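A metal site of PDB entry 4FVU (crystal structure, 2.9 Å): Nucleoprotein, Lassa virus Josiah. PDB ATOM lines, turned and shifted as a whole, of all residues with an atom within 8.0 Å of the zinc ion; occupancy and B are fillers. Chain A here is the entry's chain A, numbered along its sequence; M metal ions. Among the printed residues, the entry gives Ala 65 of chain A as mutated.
The backbone NH (N) of Leu 205 lies close to the side-chain sulfur (SG) of Cys 203, at 3.5 Å. OE1 of Glu 73 is in hydrogen-bond range of N of Ala 204 (3.0 Å). The backbone NH of Ala 65 sits at hydrogen-bond distance from the backbone carbonyl oxygen of Glu 73, at 2.9 Å. The backbone NH (N) of Met 206 sits close to the side-chain sulfur (SG) of Cys 203, 3.3 Å away. The backbone carbonyl oxygen (O) of His 105 sits at hydrogen-bond distance from a ring nitrogen (ND1) of His 183 (2.5 Å).
Merely in contact with the zinc ion: His 86 (3.8 Å). Five residues have an atom within 4 Å of the zinc ion: Glu 73, His 86, Cys 180, His 183 and Cys 203.
The zinc ion is bound by NE2 of His 183 (2.3 Å), OE2 of Glu 73 (2.4 Å), SG of Cys 180 (2.6 Å) and SG of Cys 203 (2.6 Å). The zinc ion has four donor atoms within binding distance. Slightly farther from the zinc ion lies the side-chain carboxylate (OE1) of Glu 73 (2.8 Å).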
ATOM      1  N   ALA A  65       1.905 -10.355  17.722  1.00  0.00           N
ATOM      2  CA  ALA A  65       2.553  -9.894  16.513  1.00  0.00           C
ATOM      3  C   ALA A  65       2.652 -11.108  15.585  1.00  0.00           C
ATOM      4  O   ALA A  65       2.873 -12.235  16.039  1.00  0.00           O
ATOM      5  CB  ALA A  65       3.935  -9.340  16.838  1.00  0.00           C
ATOM      6  N   GLU A  73       5.298 -13.009  17.950  1.00  0.00           N
ATOM      7  CA  GLU A  73       5.293 -12.570  19.330  1.00  0.00           C
ATOM      8  C   GLU A  73       3.929 -12.779  20.003  1.00  0.00           C
ATOM      9  O   GLU A  73       2.867 -12.562  19.395  1.00  0.00           O
ATOM     10  CB  GLU A  73       5.731 -11.120  19.383  1.00  0.00           C
ATOM     11  CG  GLU A  73       5.306 -10.435  20.604  1.00  0.00           C
ATOM     12  CD  GLU A  73       6.113  -9.222  20.879  1.00  0.00           C
ATOM     13  OE1 GLU A  73       5.981  -8.228  20.140  1.00  0.00           O
ATOM     14  OE2 GLU A  73       6.897  -9.288  21.824  1.00  0.00           O
ATOM     15  N   ILE A  74       3.955 -13.229  21.260  1.00  0.00           N
ATOM     16  CA  ILE A  74       2.725 -13.487  21.998  1.00  0.00           C
ATOM     17  C   ILE A  74       2.776 -12.959  23.429  1.00  0.00           C
ATOM     18  O   ILE A  74       3.639 -13.360  24.215  1.00  0.00           O
ATOM     19  CB  ILE A  74       2.425 -14.999  22.083  1.00  0.00           C
ATOM     20  CG1 ILE A  74       2.193 -15.581  20.687  1.00  0.00           C
ATOM     21  CG2 ILE A  74       1.236 -15.223  23.001  1.00  0.00           C
ATOM     22  CD1 ILE A  74       1.341 -16.819  20.664  1.00  0.00           C
ATOM     23  N   ALA A  75       1.847 -12.067  23.763  1.00  0.00           N
ATOM     24  CA  ALA A  75       1.728 -11.563  25.125  1.00  0.00           C
ATOM     25  C   ALA A  75       0.333 -11.728  25.711  1.00  0.00           C
ATOM     26  O   ALA A  75      -0.665 -11.638  24.989  1.00  0.00           O
ATOM     27  CB  ALA A  75       2.166 -10.122  25.236  1.00  0.00           C
ATOM     28  N   HIS A  86       4.930 -13.364  28.189  1.00  0.00           N
ATOM     29  CA  HIS A  86       5.457 -12.862  26.941  1.00  0.00           C
ATOM     30  C   HIS A  86       6.487 -13.870  26.431  1.00  0.00           C
ATOM     31  O   HIS A  86       7.368 -14.314  27.182  1.00  0.00           O
ATOM     32  CB  HIS A  86       6.115 -11.511  27.161  1.00  0.00           C
ATOM     33  CG  HIS A  86       6.710 -10.923  25.921  1.00  0.00           C
ATOM     34  ND1 HIS A  86       7.840 -10.126  25.930  1.00  0.00           N
ATOM     35  CD2 HIS A  86       6.329 -11.003  24.622  1.00  0.00           C
ATOM     36  CE1 HIS A  86       8.127  -9.751  24.705  1.00  0.00           C
ATOM     37  NE2 HIS A  86       7.232 -10.270  23.889  1.00  0.00           N
ATOM     38  N   PHE A  87       6.352 -14.246  25.164  1.00  0.00           N
ATOM     39  CA  PHE A  87       7.303 -15.142  24.528  1.00  0.00           C
ATOM     40  C   PHE A  87       7.230 -15.034  23.017  1.00  0.00           C
ATOM     41  O   PHE A  87       6.431 -14.255  22.473  1.00  0.00           O
ATOM     42  CB  PHE A  87       7.075 -16.579  24.976  1.00  0.00           C
ATOM     43  CG  PHE A  87       5.799 -17.178  24.476  1.00  0.00           C
ATOM     44  CD1 PHE A  87       5.779 -17.893  23.282  1.00  0.00           C
ATOM     45  CD2 PHE A  87       4.627 -17.036  25.210  1.00  0.00           C
ATOM     46  CE1 PHE A  87       4.598 -18.453  22.817  1.00  0.00           C
ATOM     47  CE2 PHE A  87       3.435 -17.587  24.749  1.00  0.00           C
ATOM     48  CZ  PHE A  87       3.419 -18.289  23.557  1.00  0.00           C
ATOM     49  N   PHE A  88       8.051 -15.844  22.348  1.00  0.00           N
ATOM     50  CA  PHE A  88       8.341 -15.722  20.927  1.00  0.00           C
ATOM     51  C   PHE A  88       8.398 -17.045  20.132  1.00  0.00           C
ATOM     52  O   PHE A  88       8.761 -18.107  20.667  1.00  0.00           O
ATOM     53  CB  PHE A  88       9.668 -14.979  20.739  1.00  0.00           C
ATOM     54  CG  PHE A  88       9.620 -13.529  21.172  1.00  0.00           C
ATOM     55  CD1 PHE A  88       9.103 -12.549  20.333  1.00  0.00           C
ATOM     56  CD2 PHE A  88      10.137 -13.138  22.407  1.00  0.00           C
ATOM     57  CE1 PHE A  88       9.083 -11.215  20.714  1.00  0.00           C
ATOM     58  CE2 PHE A  88      10.116 -11.803  22.788  1.00  0.00           C
ATOM     59  CZ  PHE A  88       9.589 -10.841  21.941  1.00  0.00           C
ATOM     60  N   HIS A 105       5.810  -4.675  13.054  1.00  0.00           N
ATOM     61  CA  HIS A 105       6.547  -5.021  14.276  1.00  0.00           C
ATOM     62  C   HIS A 105       8.052  -4.758  14.343  1.00  0.00           C
ATOM     63  O   HIS A 105       8.624  -4.742  15.427  1.00  0.00           O
ATOM     64  CB  HIS A 105       6.228  -6.454  14.732  1.00  0.00           C
ATOM     65  CG  HIS A 105       6.473  -7.489  13.688  1.00  0.00           C
ATOM     66  ND1 HIS A 105       5.451  -8.076  12.960  1.00  0.00           N
ATOM     67  CD2 HIS A 105       7.624  -8.066  13.248  1.00  0.00           C
ATOM     68  CE1 HIS A 105       5.967  -8.975  12.135  1.00  0.00           C
ATOM     69  NE2 HIS A 105       7.272  -8.983  12.284  1.00  0.00           N
ATOM     70  N   ILE A 107      10.543  -6.699  13.773  1.00  0.00           N
ATOM     71  CA  ILE A 107      11.319  -7.760  14.406  1.00  0.00           C
ATOM     72  C   ILE A 107      12.342  -8.379  13.434  1.00  0.00           C
ATOM     73  O   ILE A 107      12.014  -8.727  12.298  1.00  0.00           O
ATOM     74  CB  ILE A 107      10.440  -8.854  15.024  1.00  0.00           C
ATOM     75  CG1 ILE A 107       9.574  -8.265  16.138  1.00  0.00           C
ATOM     76  CG2 ILE A 107      11.280 -10.012  15.586  1.00  0.00           C
ATOM     77  CD1 ILE A 107       8.618  -9.266  16.746  1.00  0.00           C
ATOM     78  N   TRP A 173       5.866   2.906  26.526  1.00  0.00           N
ATOM     79  CA  TRP A 173       7.206   2.636  26.020  1.00  0.00           C
ATOM     80  C   TRP A 173       8.279   3.186  26.940  1.00  0.00           C
ATOM     81  O   TRP A 173       9.345   2.601  27.078  1.00  0.00           O
ATOM     82  CB  TRP A 173       7.362   3.196  24.615  1.00  0.00           C
ATOM     83  CG  TRP A 173       6.875   2.260  23.560  1.00  0.00           C
ATOM     84  CD1 TRP A 173       5.752   2.395  22.783  1.00  0.00           C
ATOM     85  CD2 TRP A 173       7.482   1.025  23.163  1.00  0.00           C
ATOM     86  NE1 TRP A 173       5.635   1.326  21.930  1.00  0.00           N
ATOM     87  CE2 TRP A 173       6.671   0.472  22.136  1.00  0.00           C
ATOM     88  CE3 TRP A 173       8.631   0.332  23.571  1.00  0.00           C
ATOM     89  CZ2 TRP A 173       6.992  -0.748  21.513  1.00  0.00           C
ATOM     90  CZ3 TRP A 173       8.941  -0.880  22.950  1.00  0.00           C
ATOM     91  CH2 TRP A 173       8.119  -1.396  21.939  1.00  0.00           C
ATOM     92  N   LEU A 179      11.410  -4.025  28.967  1.00  0.00           N
ATOM     93  CA  LEU A 179      10.677  -5.287  28.837  1.00  0.00           C
ATOM     94  C   LEU A 179      10.645  -5.844  27.427  1.00  0.00           C
ATOM     95  O   LEU A 179      10.427  -7.044  27.254  1.00  0.00           O
ATOM     96  CB  LEU A 179       9.251  -5.150  29.377  1.00  0.00           C
ATOM     97  CG  LEU A 179       9.176  -4.960  30.883  1.00  0.00           C
ATOM     98  CD1 LEU A 179       7.757  -5.223  31.393  1.00  0.00           C
ATOM     99  CD2 LEU A 179      10.190  -5.854  31.561  1.00  0.00           C
ATOM    100  N   CYS A 180      10.795  -4.997  26.410  1.00  0.00           N
ATOM    101  CA  CYS A 180      11.090  -5.524  25.081  1.00  0.00           C
ATOM    102  C   CYS A 180      12.174  -4.794  24.260  1.00  0.00           C
ATOM    103  O   CYS A 180      11.973  -3.663  23.798  1.00  0.00           O
ATOM    104  CB  CYS A 180       9.827  -5.717  24.252  1.00  0.00           C
ATOM    105  SG  CYS A 180       9.906  -7.288  23.420  1.00  0.00           S
ATOM    106  N   HIS A 181      13.288  -5.492  24.057  1.00  0.00           N
ATOM    107  CA  HIS A 181      14.369  -5.001  23.217  1.00  0.00           C
ATOM    108  C   HIS A 181      14.311  -5.607  21.825  1.00  0.00           C
ATOM    109  O   HIS A 181      15.217  -5.407  21.023  1.00  0.00           O
ATOM    110  CB  HIS A 181      15.716  -5.269  23.885  1.00  0.00           C
ATOM    111  CG  HIS A 181      15.860  -4.581  25.203  1.00  0.00           C
ATOM    112  ND1 HIS A 181      16.215  -5.249  26.358  1.00  0.00           N
ATOM    113  CD2 HIS A 181      15.698  -3.276  25.558  1.00  0.00           C
ATOM    114  CE1 HIS A 181      16.265  -4.383  27.364  1.00  0.00           C
ATOM    115  NE2 HIS A 181      15.966  -3.186  26.900  1.00  0.00           N
ATOM    116  N   MET A 182      13.248  -6.350  21.585  1.00  0.00           N
ATOM    117  CA  MET A 182      13.079  -7.196  20.404  1.00  0.00           C
ATOM    118  C   MET A 182      12.545  -6.509  19.156  1.00  0.00           C
ATOM    119  O   MET A 182      12.401  -7.150  18.116  1.00  0.00           O
ATOM    120  CB  MET A 182      12.139  -8.357  20.726  1.00  0.00           C
ATOM    121  CG  MET A 182      12.797  -9.507  21.472  1.00  0.00           C
ATOM    122  SD  MET A 182      13.755 -10.616  20.404  1.00  0.00           S
ATOM    123  CE  MET A 182      12.647 -10.787  18.995  1.00  0.00           C
ATOM    124  N   HIS A 183      12.233  -5.227  19.237  1.00  0.00           N
ATOM    125  CA  HIS A 183      11.876  -4.573  17.996  1.00  0.00           C
ATOM    126  C   HIS A 183      12.998  -3.600  17.637  1.00  0.00           C
ATOM    127  O   HIS A 183      13.044  -2.445  18.077  1.00  0.00           O
ATOM    128  CB  HIS A 183      10.528  -3.880  18.150  1.00  0.00           C
ATOM    129  CG  HIS A 183       9.467  -4.793  18.679  1.00  0.00           C
ATOM    130  ND1 HIS A 183       8.530  -5.407  17.868  1.00  0.00           N
ATOM    131  CD2 HIS A 183       9.199  -5.215  19.939  1.00  0.00           C
ATOM    132  CE1 HIS A 183       7.731  -6.156  18.605  1.00  0.00           C
ATOM    133  NE2 HIS A 183       8.123  -6.056  19.859  1.00  0.00           N
ATOM    134  N   PRO A 201       6.791   0.857  16.599  1.00  0.00           N
ATOM    135  CA  PRO A 201       6.218  -0.437  16.193  1.00  0.00           C
ATOM    136  C   PRO A 201       5.291  -1.140  17.210  1.00  0.00           C
ATOM    137  O   PRO A 201       5.040  -0.678  18.346  1.00  0.00           O
ATOM    138  CB  PRO A 201       7.458  -1.304  15.912  1.00  0.00           C
ATOM    139  CG  PRO A 201       8.566  -0.672  16.695  1.00  0.00           C
ATOM    140  CD  PRO A 201       8.266   0.793  16.764  1.00  0.00           C
ATOM    141  N   HIS A 202       4.774  -2.279  16.768  1.00  0.00           N
ATOM    142  CA  HIS A 202       3.761  -3.012  17.518  1.00  0.00           C
ATOM    143  C   HIS A 202       4.329  -4.220  18.206  1.00  0.00           C
ATOM    144  O   HIS A 202       4.586  -5.252  17.595  1.00  0.00           O
ATOM    145  CB  HIS A 202       2.640  -3.447  16.587  1.00  0.00           C
ATOM    146  CG  HIS A 202       1.856  -2.301  16.026  1.00  0.00           C
ATOM    147  ND1 HIS A 202       0.750  -2.487  15.210  1.00  0.00           N
ATOM    148  CD2 HIS A 202       2.004  -0.970  16.166  1.00  0.00           C
ATOM    149  CE1 HIS A 202       0.265  -1.307  14.873  1.00  0.00           C
ATOM    150  NE2 HIS A 202       1.016  -0.360  15.442  1.00  0.00           N
ATOM    151  N   CYS A 203       4.444  -4.083  19.522  1.00  0.00           N
ATOM    152  CA  CYS A 203       4.898  -5.100  20.441  1.00  0.00           C
ATOM    153  C   CYS A 203       3.645  -5.651  21.128  1.00  0.00           C
ATOM    154  O   CYS A 203       2.870  -4.875  21.676  1.00  0.00           O
ATOM    155  CB  CYS A 203       5.828  -4.433  21.467  1.00  0.00           C
ATOM    156  SG  CYS A 203       6.094  -5.344  22.996  1.00  0.00           S
ATOM    157  N   ALA A 204       3.442  -6.973  21.088  1.00  0.00           N
ATOM    158  CA  ALA A 204       2.273  -7.578  21.763  1.00  0.00           C
ATOM    159  C   ALA A 204       2.147  -7.101  23.205  1.00  0.00           C
ATOM    160  O   ALA A 204       1.078  -6.692  23.663  1.00  0.00           O
ATOM    161  CB  ALA A 204       2.340  -9.099  21.719  1.00  0.00           C
ATOM    162  N   LEU A 205       3.282  -7.137  23.905  1.00  0.00           N
ATOM    163  CA  LEU A 205       3.370  -6.745  25.308  1.00  0.00           C
ATOM    164  C   LEU A 205       3.021  -5.279  25.611  1.00  0.00           C
ATOM    165  O   LEU A 205       2.220  -5.020  26.510  1.00  0.00           O
ATOM    166  CB  LEU A 205       4.764  -7.091  25.857  1.00  0.00           C
ATOM    167  CG  LEU A 205       4.761  -7.104  27.387  1.00  0.00           C
ATOM    168  CD1 LEU A 205       3.580  -7.957  27.893  1.00  0.00           C
ATOM    169  CD2 LEU A 205       6.098  -7.584  27.970  1.00  0.00           C
ATOM    170  N   MET A 206       3.617  -4.347  24.890  1.00  0.00           N
ATOM    171  CA  MET A 206       3.317  -2.919  25.088  1.00  0.00           C
ATOM    172  C   MET A 206       1.846  -2.617  24.775  1.00  0.00           C
ATOM    173  O   MET A 206       1.170  -1.888  25.507  1.00  0.00           O
ATOM    174  CB  MET A 206       4.223  -2.032  24.226  1.00  0.00           C
ATOM    175  CG  MET A 206       5.706  -2.115  24.582  1.00  0.00           C
ATOM    176  SD  MET A 206       6.101  -2.030  26.346  1.00  0.00           S
ATOM    177  CE  MET A 206       7.872  -2.369  26.325  1.00  0.00           C
ATOM    178  N   ASP A 207       1.380  -3.189  23.667  1.00  0.00           N
ATOM    179  CA  ASP A 207      -0.015  -3.067  23.269  1.00  0.00           C
ATOM    180  C   ASP A 207      -0.936  -3.545  24.379  1.00  0.00           C
ATOM    181  O   ASP A 207      -1.928  -2.893  24.691  1.00  0.00           O
ATOM    182  CB  ASP A 207      -0.277  -3.861  21.995  1.00  0.00           C
ATOM    183  CG  ASP A 207       0.381  -3.254  20.773  1.00  0.00           C
ATOM    184  OD1 ASP A 207       1.394  -2.533  20.951  1.00  0.00           O
ATOM    185  OD2 ASP A 207      -0.113  -3.509  19.651  1.00  0.00           O
HETATM  186 ZN    ZN M   1       7.782  -7.055  21.917  1.00  0.00          ZN
